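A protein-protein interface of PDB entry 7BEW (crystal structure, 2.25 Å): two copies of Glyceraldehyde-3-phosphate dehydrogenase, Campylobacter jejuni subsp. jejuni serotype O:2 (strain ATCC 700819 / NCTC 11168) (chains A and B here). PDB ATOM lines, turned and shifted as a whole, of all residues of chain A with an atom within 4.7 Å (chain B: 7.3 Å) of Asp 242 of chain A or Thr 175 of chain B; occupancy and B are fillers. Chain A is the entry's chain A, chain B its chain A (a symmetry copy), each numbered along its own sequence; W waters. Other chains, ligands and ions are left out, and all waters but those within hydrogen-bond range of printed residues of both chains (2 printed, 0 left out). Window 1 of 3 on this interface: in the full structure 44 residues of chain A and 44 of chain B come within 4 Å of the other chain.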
ATOM      1  N   LEU A 173      29.622 -20.366 -19.098  1.00  0.00           N
ATOM      2  CA  LEU A 173      28.836 -21.598 -18.944  1.00  0.00           C
ATOM      3  C   LEU A 173      27.380 -21.191 -18.768  1.00  0.00           C
ATOM      4  O   LEU A 173      27.079 -20.116 -18.260  1.00  0.00           O
ATOM      5  CB  LEU A 173      29.354 -22.428 -17.766  1.00  0.00           C
ATOM      6  CG  LEU A 173      30.755 -23.017 -17.926  1.00  0.00           C
ATOM      7  CD1 LEU A 173      31.340 -23.493 -16.590  1.00  0.00           C
ATOM      8  CD2 LEU A 173      30.741 -24.135 -18.954  1.00  0.00           C
ATOM      9  N   MET A 174      26.508 -22.033 -19.241  1.00  0.00           N
ATOM     10  CA  MET A 174      25.090 -21.706 -19.389  1.00  0.00           C
ATOM     11  C   MET A 174      24.319 -22.842 -18.729  1.00  0.00           C
ATOM     12  O   MET A 174      24.714 -24.009 -18.921  1.00  0.00           O
ATOM     13  CB  MET A 174      24.791 -21.605 -20.884  1.00  0.00           C
ATOM     14  CG  MET A 174      23.359 -21.331 -21.173  1.00  0.00           C
ATOM     15  SD  MET A 174      22.678 -22.331 -22.521  1.00  0.00           S
ATOM     16  CE  MET A 174      22.995 -23.978 -21.900  1.00  0.00           C
ATOM     17  N   THR A 175      23.282 -22.507 -17.961  1.00  0.00           N
ATOM     18  CA  THR A 175      22.180 -23.434 -17.608  1.00  0.00           C
ATOM     19  C   THR A 175      20.885 -22.927 -18.237  1.00  0.00           C
ATOM     20  O   THR A 175      20.632 -21.706 -18.223  1.00  0.00           O
ATOM     21  CB  THR A 175      21.997 -23.569 -16.093  1.00  0.00           C
ATOM     22  OG1 THR A 175      23.280 -23.969 -15.615  1.00  0.00           O
ATOM     23  CG2 THR A 175      20.903 -24.552 -15.702  1.00  0.00           C
ATOM     24  N   SER A 240      14.211 -20.471 -19.684  1.00  0.00           N
ATOM     25  CA  SER A 240      15.201 -19.386 -19.485  1.00  0.00           C
ATOM     26  C   SER A 240      16.611 -19.868 -19.787  1.00  0.00           C
ATOM     27  O   SER A 240      16.959 -21.032 -19.529  1.00  0.00           O
ATOM     28  CB  SER A 240      15.152 -18.799 -18.116  1.00  0.00           C
ATOM     29  OG  SER A 240      14.980 -19.809 -17.149  1.00  0.00           O
ATOM     30  N   VAL A 241      17.383 -18.960 -20.343  1.00  0.00           N
ATOM     31  CA  VAL A 241      18.851 -19.088 -20.432  1.00  0.00           C
ATOM     32  C   VAL A 241      19.425 -18.313 -19.260  1.00  0.00           C
ATOM     33  O   VAL A 241      19.022 -17.150 -19.065  1.00  0.00           O
ATOM     34  CB  VAL A 241      19.406 -18.540 -21.748  1.00  0.00           C
ATOM     35  CG1 VAL A 241      20.915 -18.364 -21.649  1.00  0.00           C
ATOM     36  CG2 VAL A 241      19.036 -19.437 -22.908  1.00  0.00           C
ATOM     37  N   ASP A 242      20.311 -18.972 -18.524  1.00  0.00           N
ATOM     38  CA  ASP A 242      21.126 -18.392 -17.438  1.00  0.00           C
ATOM     39  C   ASP A 242      22.584 -18.488 -17.893  1.00  0.00           C
ATOM     40  O   ASP A 242      23.180 -19.577 -17.817  1.00  0.00           O
ATOM     41  CB  ASP A 242      20.765 -19.131 -16.154  1.00  0.00           C
ATOM     42  CG  ASP A 242      21.580 -18.782 -14.929  1.00  0.00           C
ATOM     43  OD1 ASP A 242      22.691 -18.203 -15.094  1.00  0.00           O
ATOM     44  OD2 ASP A 242      21.112 -19.141 -13.819  1.00  0.00           O
ATOM     45  N   LEU A 243      23.107 -17.410 -18.444  1.00  0.00           N
ATOM     46  CA  LEU A 243      24.487 -17.360 -18.964  1.00  0.00           C
ATOM     47  C   LEU A 243      25.391 -16.722 -17.925  1.00  0.00           C
ATOM     48  O   LEU A 243      25.185 -15.561 -17.617  1.00  0.00           O
ATOM     49  CB  LEU A 243      24.518 -16.516 -20.235  1.00  0.00           C
ATOM     50  CG  LEU A 243      25.910 -16.399 -20.832  1.00  0.00           C
ATOM     51  CD1 LEU A 243      26.457 -17.788 -21.184  1.00  0.00           C
ATOM     52  CD2 LEU A 243      25.910 -15.471 -22.040  1.00  0.00           C
ATOM     53  N   THR A 244      26.432 -17.431 -17.525  1.00  0.00           N
ATOM     54  CA  THR A 244      27.490 -16.889 -16.664  1.00  0.00           C
ATOM     55  C   THR A 244      28.770 -16.784 -17.488  1.00  0.00           C
ATOM     56  O   THR A 244      29.192 -17.752 -18.036  1.00  0.00           O
ATOM     57  CB  THR A 244      27.615 -17.720 -15.391  1.00  0.00           C
ATOM     58  OG1 THR A 244      26.331 -17.896 -14.785  1.00  0.00           O
ATOM     59  CG2 THR A 244      28.537 -17.051 -14.398  1.00  0.00           C
ATOM     60  N   LYS A 307      26.288 -12.510 -14.957  1.00  0.00           N
ATOM     61  CA  LYS A 307      25.149 -13.394 -15.200  1.00  0.00           C
ATOM     62  C   LYS A 307      24.060 -12.616 -15.921  1.00  0.00           C
ATOM     63  O   LYS A 307      23.741 -11.485 -15.487  1.00  0.00           O
ATOM     64  CB  LYS A 307      24.573 -13.920 -13.894  1.00  0.00           C
ATOM     65  CG  LYS A 307      23.590 -15.071 -14.076  1.00  0.00           C
ATOM     66  CD  LYS A 307      22.979 -15.555 -12.789  1.00  0.00           C
ATOM     67  CE  LYS A 307      23.905 -16.393 -11.937  1.00  0.00           C
ATOM     68  NZ  LYS A 307      24.099 -17.762 -12.478  1.00  0.00           N
ATOM     69  N   VAL A 308      23.508 -13.215 -16.971  1.00  0.00           N
ATOM     70  CA  VAL A 308      22.336 -12.702 -17.728  1.00  0.00           C
ATOM     71  C   VAL A 308      21.250 -13.787 -17.790  1.00  0.00           C
ATOM     72  O   VAL A 308      21.580 -14.939 -18.080  1.00  0.00           O
ATOM     73  CB  VAL A 308      22.770 -12.278 -19.138  1.00  0.00           C
ATOM     74  CG1 VAL A 308      21.554 -12.088 -20.006  1.00  0.00           C
ATOM     75  CG2 VAL A 308      23.597 -11.010 -19.110  1.00  0.00           C
ATOM     76  N   ILE A 309      20.013 -13.426 -17.475  1.00  0.00           N
ATOM     77  CA  ILE A 309      18.814 -14.313 -17.521  1.00  0.00           C
ATOM     78  C   ILE A 309      17.913 -13.788 -18.625  1.00  0.00           C
ATOM     79  O   ILE A 309      17.527 -12.582 -18.576  1.00  0.00           O
ATOM     80  CB  ILE A 309      18.016 -14.368 -16.201  1.00  0.00           C
ATOM     81  CG1 ILE A 309      18.885 -14.540 -14.952  1.00  0.00           C
ATOM     82  CG2 ILE A 309      16.961 -15.460 -16.276  1.00  0.00           C
ATOM     83  CD1 ILE A 309      19.728 -15.764 -14.978  1.00  0.00           C
ATOM     84  N   THR B 152      19.909 -22.866   1.614  1.00  0.00           N
ATOM     85  CA  THR B 152      20.858 -22.600   0.512  1.00  0.00           C
ATOM     86  C   THR B 152      22.280 -22.462   1.059  1.00  0.00           C
ATOM     87  O   THR B 152      23.202 -23.001   0.449  1.00  0.00           O
ATOM     88  CB  THR B 152      20.392 -21.401  -0.309  1.00  0.00           C
ATOM     89  OG1 THR B 152      19.111 -21.742  -0.841  1.00  0.00           O
ATOM     90  CG2 THR B 152      21.347 -21.077  -1.436  1.00  0.00           C
ATOM     91  N   LEU B 173      29.143 -16.754  -9.304  1.00  0.00           N
ATOM     92  CA  LEU B 173      27.717 -16.406  -9.240  1.00  0.00           C
ATOM     93  C   LEU B 173      26.931 -17.709  -9.195  1.00  0.00           C
ATOM     94  O   LEU B 173      27.367 -18.730  -9.717  1.00  0.00           O
ATOM     95  CB  LEU B 173      27.319 -15.528 -10.430  1.00  0.00           C
ATOM     96  CG  LEU B 173      27.939 -14.131 -10.469  1.00  0.00           C
ATOM     97  CD1 LEU B 173      27.804 -13.475 -11.849  1.00  0.00           C
ATOM     98  CD2 LEU B 173      27.338 -13.259  -9.381  1.00  0.00           C
ATOM     99  N   MET B 174      25.817 -17.660  -8.526  1.00  0.00           N
ATOM    100  CA  MET B 174      25.058 -18.857  -8.165  1.00  0.00           C
ATOM    101  C   MET B 174      23.622 -18.603  -8.606  1.00  0.00           C
ATOM    102  O   MET B 174      23.137 -17.473  -8.406  1.00  0.00           O
ATOM    103  CB  MET B 174      25.166 -19.035  -6.650  1.00  0.00           C
ATOM    104  CG  MET B 174      24.385 -20.193  -6.144  1.00  0.00           C
ATOM    105  SD  MET B 174      23.444 -19.841  -4.636  1.00  0.00           S
ATOM    106  CE  MET B 174      22.439 -18.469  -5.189  1.00  0.00           C
ATOM    107  N   THR B 175      22.985 -19.607  -9.210  1.00  0.00           N
ATOM    108  CA  THR B 175      21.509 -19.710  -9.309  1.00  0.00           C
ATOM    109  C   THR B 175      21.042 -20.922  -8.506  1.00  0.00           C
ATOM    110  O   THR B 175      21.695 -21.983  -8.560  1.00  0.00           O
ATOM    111  CB  THR B 175      21.032 -19.839 -10.759  1.00  0.00           C
ATOM    112  OG1 THR B 175      21.590 -18.704 -11.418  1.00  0.00           O
ATOM    113  CG2 THR B 175      19.517 -19.899 -10.893  1.00  0.00           C
ATOM    114  N   THR B 176      19.942 -20.775  -7.794  1.00  0.00           N
ATOM    115  CA  THR B 176      19.271 -21.924  -7.168  1.00  0.00           C
ATOM    116  C   THR B 176      17.976 -22.127  -7.925  1.00  0.00           C
ATOM    117  O   THR B 176      17.253 -21.165  -8.159  1.00  0.00           O
ATOM    118  CB  THR B 176      19.054 -21.755  -5.660  1.00  0.00           C
ATOM    119  OG1 THR B 176      18.409 -20.521  -5.389  1.00  0.00           O
ATOM    120  CG2 THR B 176      20.340 -21.684  -4.882  1.00  0.00           C
ATOM    121  N   ILE B 177      17.732 -23.362  -8.307  1.00  0.00           N
ATOM    122  CA  ILE B 177      16.395 -23.787  -8.760  1.00  0.00           C
ATOM    123  C   ILE B 177      15.701 -24.347  -7.536  1.00  0.00           C
ATOM    124  O   ILE B 177      16.164 -25.372  -7.006  1.00  0.00           O
ATOM    125  CB  ILE B 177      16.513 -24.787  -9.903  1.00  0.00           C
ATOM    126  CG1 ILE B 177      17.296 -24.156 -11.056  1.00  0.00           C
ATOM    127  CG2 ILE B 177      15.116 -25.259 -10.271  1.00  0.00           C
ATOM    128  CD1 ILE B 177      17.865 -25.148 -12.015  1.00  0.00           C
ATOM    129  N   HIS B 178      14.710 -23.622  -7.052  1.00  0.00           N
ATOM    130  CA  HIS B 178      14.178 -23.847  -5.700  1.00  0.00           C
ATOM    131  C   HIS B 178      12.706 -24.261  -5.771  1.00  0.00           C
ATOM    132  O   HIS B 178      11.925 -23.634  -6.527  1.00  0.00           O
ATOM    133  CB  HIS B 178      14.423 -22.594  -4.865  1.00  0.00           C
ATOM    134  CG  HIS B 178      14.449 -22.827  -3.395  1.00  0.00           C
ATOM    135  ND1 HIS B 178      13.317 -23.179  -2.696  1.00  0.00           N
ATOM    136  CD2 HIS B 178      15.465 -22.754  -2.498  1.00  0.00           C
ATOM    137  CE1 HIS B 178      13.617 -23.299  -1.415  1.00  0.00           C
ATOM    138  NE2 HIS B 178      14.940 -23.039  -1.256  1.00  0.00           N
ATOM    139  N   THR B 209      17.959 -13.983  -3.293  1.00  0.00           N
ATOM    140  CA  THR B 209      18.549 -14.650  -2.101  1.00  0.00           C
ATOM    141  C   THR B 209      19.853 -13.927  -1.757  1.00  0.00           C
ATOM    142  O   THR B 209      20.675 -13.639  -2.687  1.00  0.00           O
ATOM    143  CB  THR B 209      18.757 -16.166  -2.300  1.00  0.00           C
ATOM    144  OG1 THR B 209      19.604 -16.645  -1.255  1.00  0.00           O
ATOM    145  CG2 THR B 209      19.442 -16.569  -3.586  1.00  0.00           C
ATOM    146  N   HIS B 227      27.936 -13.690  -5.494  1.00  0.00           N
ATOM    147  CA  HIS B 227      26.522 -13.247  -5.433  1.00  0.00           C
ATOM    148  C   HIS B 227      25.691 -14.320  -6.129  1.00  0.00           C
ATOM    149  O   HIS B 227      26.255 -15.293  -6.645  1.00  0.00           O
ATOM    150  CB  HIS B 227      26.365 -11.832  -6.012  1.00  0.00           C
ATOM    151  CG  HIS B 227      25.158 -11.117  -5.510  1.00  0.00           C
ATOM    152  ND1 HIS B 227      24.292 -11.675  -4.581  1.00  0.00           N
ATOM    153  CD2 HIS B 227      24.676  -9.887  -5.763  1.00  0.00           C
ATOM    154  CE1 HIS B 227      23.315 -10.838  -4.321  1.00  0.00           C
ATOM    155  NE2 HIS B 227      23.533  -9.739  -5.017  1.00  0.00           N
ATOM    156  N   GLY B 228      24.386 -14.197  -6.080  1.00  0.00           N
ATOM    157  CA  GLY B 228      23.526 -15.154  -6.775  1.00  0.00           C
ATOM    158  C   GLY B 228      22.076 -14.796  -6.643  1.00  0.00           C
ATOM    159  O   GLY B 228      21.747 -13.676  -6.164  1.00  0.00           O
ATOM    160  N   GLN B 229      21.239 -15.714  -7.117  1.00  0.00           N
ATOM    161  CA  GLN B 229      19.792 -15.468  -7.232  1.00  0.00           C
ATOM    162  C   GLN B 229      19.087 -16.808  -7.312  1.00  0.00           C
ATOM    163  O   GLN B 229      19.771 -17.802  -7.326  1.00  0.00           O
ATOM    164  CB  GLN B 229      19.510 -14.509  -8.397  1.00  0.00           C
ATOM    165  CG  GLN B 229      19.881 -15.062  -9.766  1.00  0.00           C
ATOM    166  CD  GLN B 229      19.608 -14.026 -10.830  1.00  0.00           C
ATOM    167  OE1 GLN B 229      20.506 -13.304 -11.292  1.00  0.00           O
ATOM    168  NE2 GLN B 229      18.344 -13.928 -11.192  1.00  0.00           N
ATOM    169  N   SER B 230      17.753 -16.790  -7.362  1.00  0.00           N
ATOM    170  CA  SER B 230      16.903 -17.992  -7.291  1.00  0.00           C
ATOM    171  C   SER B 230      15.835 -17.977  -8.389  1.00  0.00           C
ATOM    172  O   SER B 230      15.381 -16.891  -8.831  1.00  0.00           O
ATOM    173  CB  SER B 230      16.319 -18.103  -5.910  1.00  0.00           C
ATOM    174  OG  SER B 230      15.616 -19.325  -5.764  1.00  0.00           O
ATOM    175  N   MET B 231      15.446 -19.170  -8.819  1.00  0.00           N
ATOM    176  CA  MET B 231      14.294 -19.415  -9.722  1.00  0.00           C
ATOM    177  C   MET B 231      13.402 -20.453  -9.030  1.00  0.00           C
ATOM    178  O   MET B 231      13.817 -21.624  -8.855  1.00  0.00           O
ATOM    179  CB  MET B 231      14.769 -19.920 -11.090  1.00  0.00           C
ATOM    180  CG  MET B 231      15.706 -18.955 -11.823  1.00  0.00           C
ATOM    181  SD  MET B 231      14.893 -17.419 -12.392  1.00  0.00           S
ATOM    182  CE  MET B 231      14.690 -17.735 -14.154  1.00  0.00           C
ATOM    183  N   SER B 240      18.224 -27.171  -6.125  1.00  0.00           N
ATOM    184  CA  SER B 240      19.635 -27.296  -6.559  1.00  0.00           C
ATOM    185  C   SER B 240      20.358 -25.962  -6.468  1.00  0.00           C
ATOM    186  O   SER B 240      19.766 -24.896  -6.702  1.00  0.00           O
ATOM    187  CB  SER B 240      19.771 -27.849  -7.937  1.00  0.00           C
ATOM    188  OG  SER B 240      18.796 -27.297  -8.791  1.00  0.00           O
ATOM    189  N   VAL B 241      21.620 -26.057  -6.113  1.00  0.00           N
ATOM    190  CA  VAL B 241      22.591 -24.954  -6.263  1.00  0.00           C
ATOM    191  C   VAL B 241      23.331 -25.204  -7.565  1.00  0.00           C
ATOM    192  O   VAL B 241      23.806 -26.338  -7.767  1.00  0.00           O
ATOM    193  CB  VAL B 241      23.581 -24.885  -5.100  1.00  0.00           C
ATOM    194  CG1 VAL B 241      24.757 -23.988  -5.464  1.00  0.00           C
ATOM    195  CG2 VAL B 241      22.901 -24.408  -3.837  1.00  0.00           C
ATOM    196  N   ASP B 242      23.386 -24.169  -8.393  1.00  0.00           N
ATOM    197  CA  ASP B 242      24.178 -24.107  -9.638  1.00  0.00           C
ATOM    198  C   ASP B 242      25.224 -23.010  -9.430  1.00  0.00           C
ATOM    199  O   ASP B 242      24.891 -21.816  -9.532  1.00  0.00           O
ATOM    200  CB  ASP B 242      23.200 -23.903 -10.790  1.00  0.00           C
ATOM    201  CG  ASP B 242      23.811 -23.682 -12.155  1.00  0.00           C
ATOM    202  OD1 ASP B 242      25.024 -23.333 -12.219  1.00  0.00           O
ATOM    203  OD2 ASP B 242      23.047 -23.816 -13.145  1.00  0.00           O
ATOM    204  N   LEU B 243      26.426 -23.400  -9.049  1.00  0.00           N
ATOM    205  CA  LEU B 243      27.527 -22.457  -8.773  1.00  0.00           C
ATOM    206  C   LEU B 243      28.430 -22.373  -9.990  1.00  0.00           C
ATOM    207  O   LEU B 243      29.026 -23.379 -10.336  1.00  0.00           O
ATOM    208  CB  LEU B 243      28.341 -22.964  -7.585  1.00  0.00           C
ATOM    209  CG  LEU B 243      29.511 -22.058  -7.241  1.00  0.00           C
ATOM    210  CD1 LEU B 243      29.008 -20.650  -6.893  1.00  0.00           C
ATOM    211  CD2 LEU B 243      30.347 -22.651  -6.115  1.00  0.00           C
ATOM    212  N   THR B 244      28.618 -21.173 -10.512  1.00  0.00           N
ATOM    213  CA  THR B 244      29.595 -20.902 -11.573  1.00  0.00           C
ATOM    214  C   THR B 244      30.715 -20.049 -10.985  1.00  0.00           C
ATOM    215  O   THR B 244      30.446 -19.019 -10.451  1.00  0.00           O
ATOM    216  CB  THR B 244      28.901 -20.299 -12.790  1.00  0.00           C
ATOM    217  OG1 THR B 244      27.767 -21.089 -13.157  1.00  0.00           O
ATOM    218  CG2 THR B 244      29.847 -20.222 -13.967  1.00  0.00           C
ATOM    219  N   LYS B 307      31.447 -25.022 -13.344  1.00  0.00           N
ATOM    220  CA  LYS B 307      30.074 -25.142 -12.853  1.00  0.00           C
ATOM    221  C   LYS B 307      29.954 -26.403 -12.013  1.00  0.00           C
ATOM    222  O   LYS B 307      30.427 -27.471 -12.462  1.00  0.00           O
ATOM    223  CB  LYS B 307      29.085 -25.240 -14.005  1.00  0.00           C
ATOM    224  CG  LYS B 307      27.631 -25.064 -13.583  1.00  0.00           C
ATOM    225  CD  LYS B 307      26.651 -25.216 -14.713  1.00  0.00           C
ATOM    226  CE  LYS B 307      26.591 -24.031 -15.650  1.00  0.00           C
ATOM    227  NZ  LYS B 307      25.885 -22.867 -15.059  1.00  0.00           N
ATOM    228  N   VAL B 308      29.329 -26.274 -10.847  1.00  0.00           N
ATOM    229  CA  VAL B 308      28.975 -27.396  -9.940  1.00  0.00           C
ATOM    230  C   VAL B 308      27.472 -27.346  -9.623  1.00  0.00           C
ATOM    231  O   VAL B 308      26.968 -26.263  -9.316  1.00  0.00           O
ATOM    232  CB  VAL B 308      29.810 -27.313  -8.655  1.00  0.00           C
ATOM    233  CG1 VAL B 308      29.223 -28.224  -7.609  1.00  0.00           C
ATOM    234  CG2 VAL B 308      31.260 -27.672  -8.906  1.00  0.00           C
ATOM    235  N   ILE B 309      26.788 -28.476  -9.748  1.00  0.00           N
ATOM    236  CA  ILE B 309      25.338 -28.646  -9.442  1.00  0.00           C
ATOM    237  C   ILE B 309      25.242 -29.570  -8.240  1.00  0.00           C
ATOM    238  O   ILE B 309      25.785 -30.713  -8.304  1.00  0.00           O
ATOM    239  CB  ILE B 309      24.511 -29.241 -10.602  1.00  0.00           C
ATOM    240  CG1 ILE B 309      24.801 -28.606 -11.965  1.00  0.00           C
ATOM    241  CG2 ILE B 309      23.028 -29.163 -10.277  1.00  0.00           C
ATOM    242  CD1 ILE B 309      24.566 -27.138 -11.998  1.00  0.00           C
ATOM    243  N   TYR B 312      19.727 -30.250  -2.753  1.00  0.00           N
ATOM    244  CA  TYR B 312      19.416 -30.250  -1.308  1.00  0.00           C
ATOM    245  C   TYR B 312      17.912 -30.379  -1.100  1.00  0.00           C
ATOM    246  O   TYR B 312      17.126 -29.691  -1.772  1.00  0.00           O
ATOM    247  CB  TYR B 312      20.014 -29.017  -0.650  1.00  0.00           C
ATOM    248  CG  TYR B 312      19.601 -27.664  -1.163  1.00  0.00           C
ATOM    249  CD1 TYR B 312      19.989 -27.208  -2.410  1.00  0.00           C
ATOM    250  CD2 TYR B 312      18.967 -26.774  -0.321  1.00  0.00           C
ATOM    251  CE1 TYR B 312      19.638 -25.941  -2.859  1.00  0.00           C
ATOM    252  CE2 TYR B 312      18.608 -25.499  -0.744  1.00  0.00           C
ATOM    253  CZ  TYR B 312      18.942 -25.074  -2.024  1.00  0.00           C
ATOM    254  OH  TYR B 312      18.617 -23.796  -2.421  1.00  0.00           O
HETATM  255  O   HOH W   1      25.095 -20.079 -15.673  1.00  0.00           O
HETATM  256  O   HOH W   2      25.547 -20.287 -11.928  1.00  0.00           O
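The side-chain carboxylate of Asp 242 of chain B lies within hydrogen-bond range of the side-chain hydroxyl of Thr 175 of chain A (2.5 Å). The side-chain hydroxyl (OG1) of Thr 175 of chain A sits at hydrogen-bond distance from the side-chain amino group (NZ) of Lys 307 of chain B (2.9 Å). The side-chain hydroxyl of Thr 175 of chain B sits at hydrogen-bond distance from the side-chain carboxylate of Asp 242 of chain A (2.5 Å). OG1 of Thr 175 of chain B lies within hydrogen-bond range of NZ of Lys 307 of chain A.
The backbone NH (N) of Leu 173 of chain A is in hydrogen-bond range of the backbone carbonyl oxygen (O) of Thr 244 of chain A, at 2.9 Å. The backbone NH (N) of Asp 242 of chain A is in hydrogen-bond range of the backbone carbonyl oxygen (O) of Thr 175 of chain A (2.8 Å). The side-chain hydroxyl (OG1) of Thr 244 of chain A sits at hydrogen-bond distance from the side-chain amino group (NZ) of Lys 307 of chain A, at 3.2 Å. The backbone NH (N) of Thr 176 of chain B sits at hydrogen-bond distance from the backbone carbonyl oxygen (O) of Gln 229 of chain B (3.0 Å). The backbone carbonyl oxygen (O) of Thr 176 of chain B lies within hydrogen-bond range of the backbone NH (N) of Met 231 of chain B. The side-chain hydroxyl (OG1) of Thr 244 of chain B is in hydrogen-bond range of the side-chain amino group (NZ) of Lys 307 of chain B (3.2 Å).
Among the printed residues, merely in contact across the chains: Thr 244 of chain A with Thr 244 of chain B, Leu 173 of chain A with Lys 307 of chain B, Lys 307 of chain A with Leu 173 of chain B, Ser 240 of chain A with Met 231 of chain B, Lys 307 of chain A with Gln 229 of chain B, Met 174 of chain A with Lys 307 of chain B, Lys 307 of chain A with Met 174 of chain B, Ile 309 of chain A with Gln 229 of chain B and Ile 309 of chain A with Met 231 of chain B.
Asp 242 of chain A touches just one residue of chain B: Thr 175 (2.5 Å). Of the printed residues of chain B, Ile 309 of chain A touches Gln 229 and Met 231. Of the printed residues of chain A, Leu 173 of chain B touches Lys 307 (3.6 Å). Of chain A, only Asp 242 and Lys 307 come within 4 Å of Thr 175 of chain B. Thr 209 of chain B touches none of the printed residues of chain A. Of the printed residues of chain A, Met 231 of chain B touches Ser 240 and Ile 309. Ser 240 of chain B touches none of the printed residues of chain A. The nearest residue of chain B that does not touch Asp 242 of chain A is Lys 307 of chain B (5.1 Å). The nearest printed residue of chain A that does not touch Thr 175 of chain B is Ile 309 of chain A (5.0 Å). The nearest printed residue of chain B that does not touch Leu 173 of chain A is Thr 244 of chain B (4.4 Å).
Of the 22 printed residues of chain B, 8 touch a printed residue of chain A. Among the printed residues, 13 pairs touch across the chains.
Leu 173 of chain A touches Lys 307 of chain B, and with the chains exchanged Lys 307 of chain A touches Leu 173 of chain B. Met 174 of chain A touches Lys 307 of chain B, and with the chains exchanged Lys 307 of chain A touches Met 174 of chain B. Thr 175 of chain A touches Asp 242 of chain B, and with the chains exchanged Asp 242 of chain A touches Thr 175 of chain B. Thr 244 of chain B touches its own counterpart, Thr 244 of chain A. Positions printed for both chains: 173, 174, 175, 240, 241, 242, 243, 244, 307, 308 and 309. Of the 13 pairs that touch across the chains among the printed residues, 9 have their exchanged pair printed and touching as well.
Water W1 lies within hydrogen-bond range of OG1 of Thr 244 of chain A (2.7 Å), O of Asp 242 of chain A (2.9 Å), NZ of Lys 307 of chain B (3.0 Å) and O of Leu 173 of chain A (3.3 Å). Water W2 lies within hydrogen-bond range of OG1 of Thr 244 of chain B (2.7 Å), O of Asp 242 of chain B (2.9 Å), NZ of Lys 307 of chain A (3.0 Å) and O of Leu 173 of chain B (3.3 Å).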
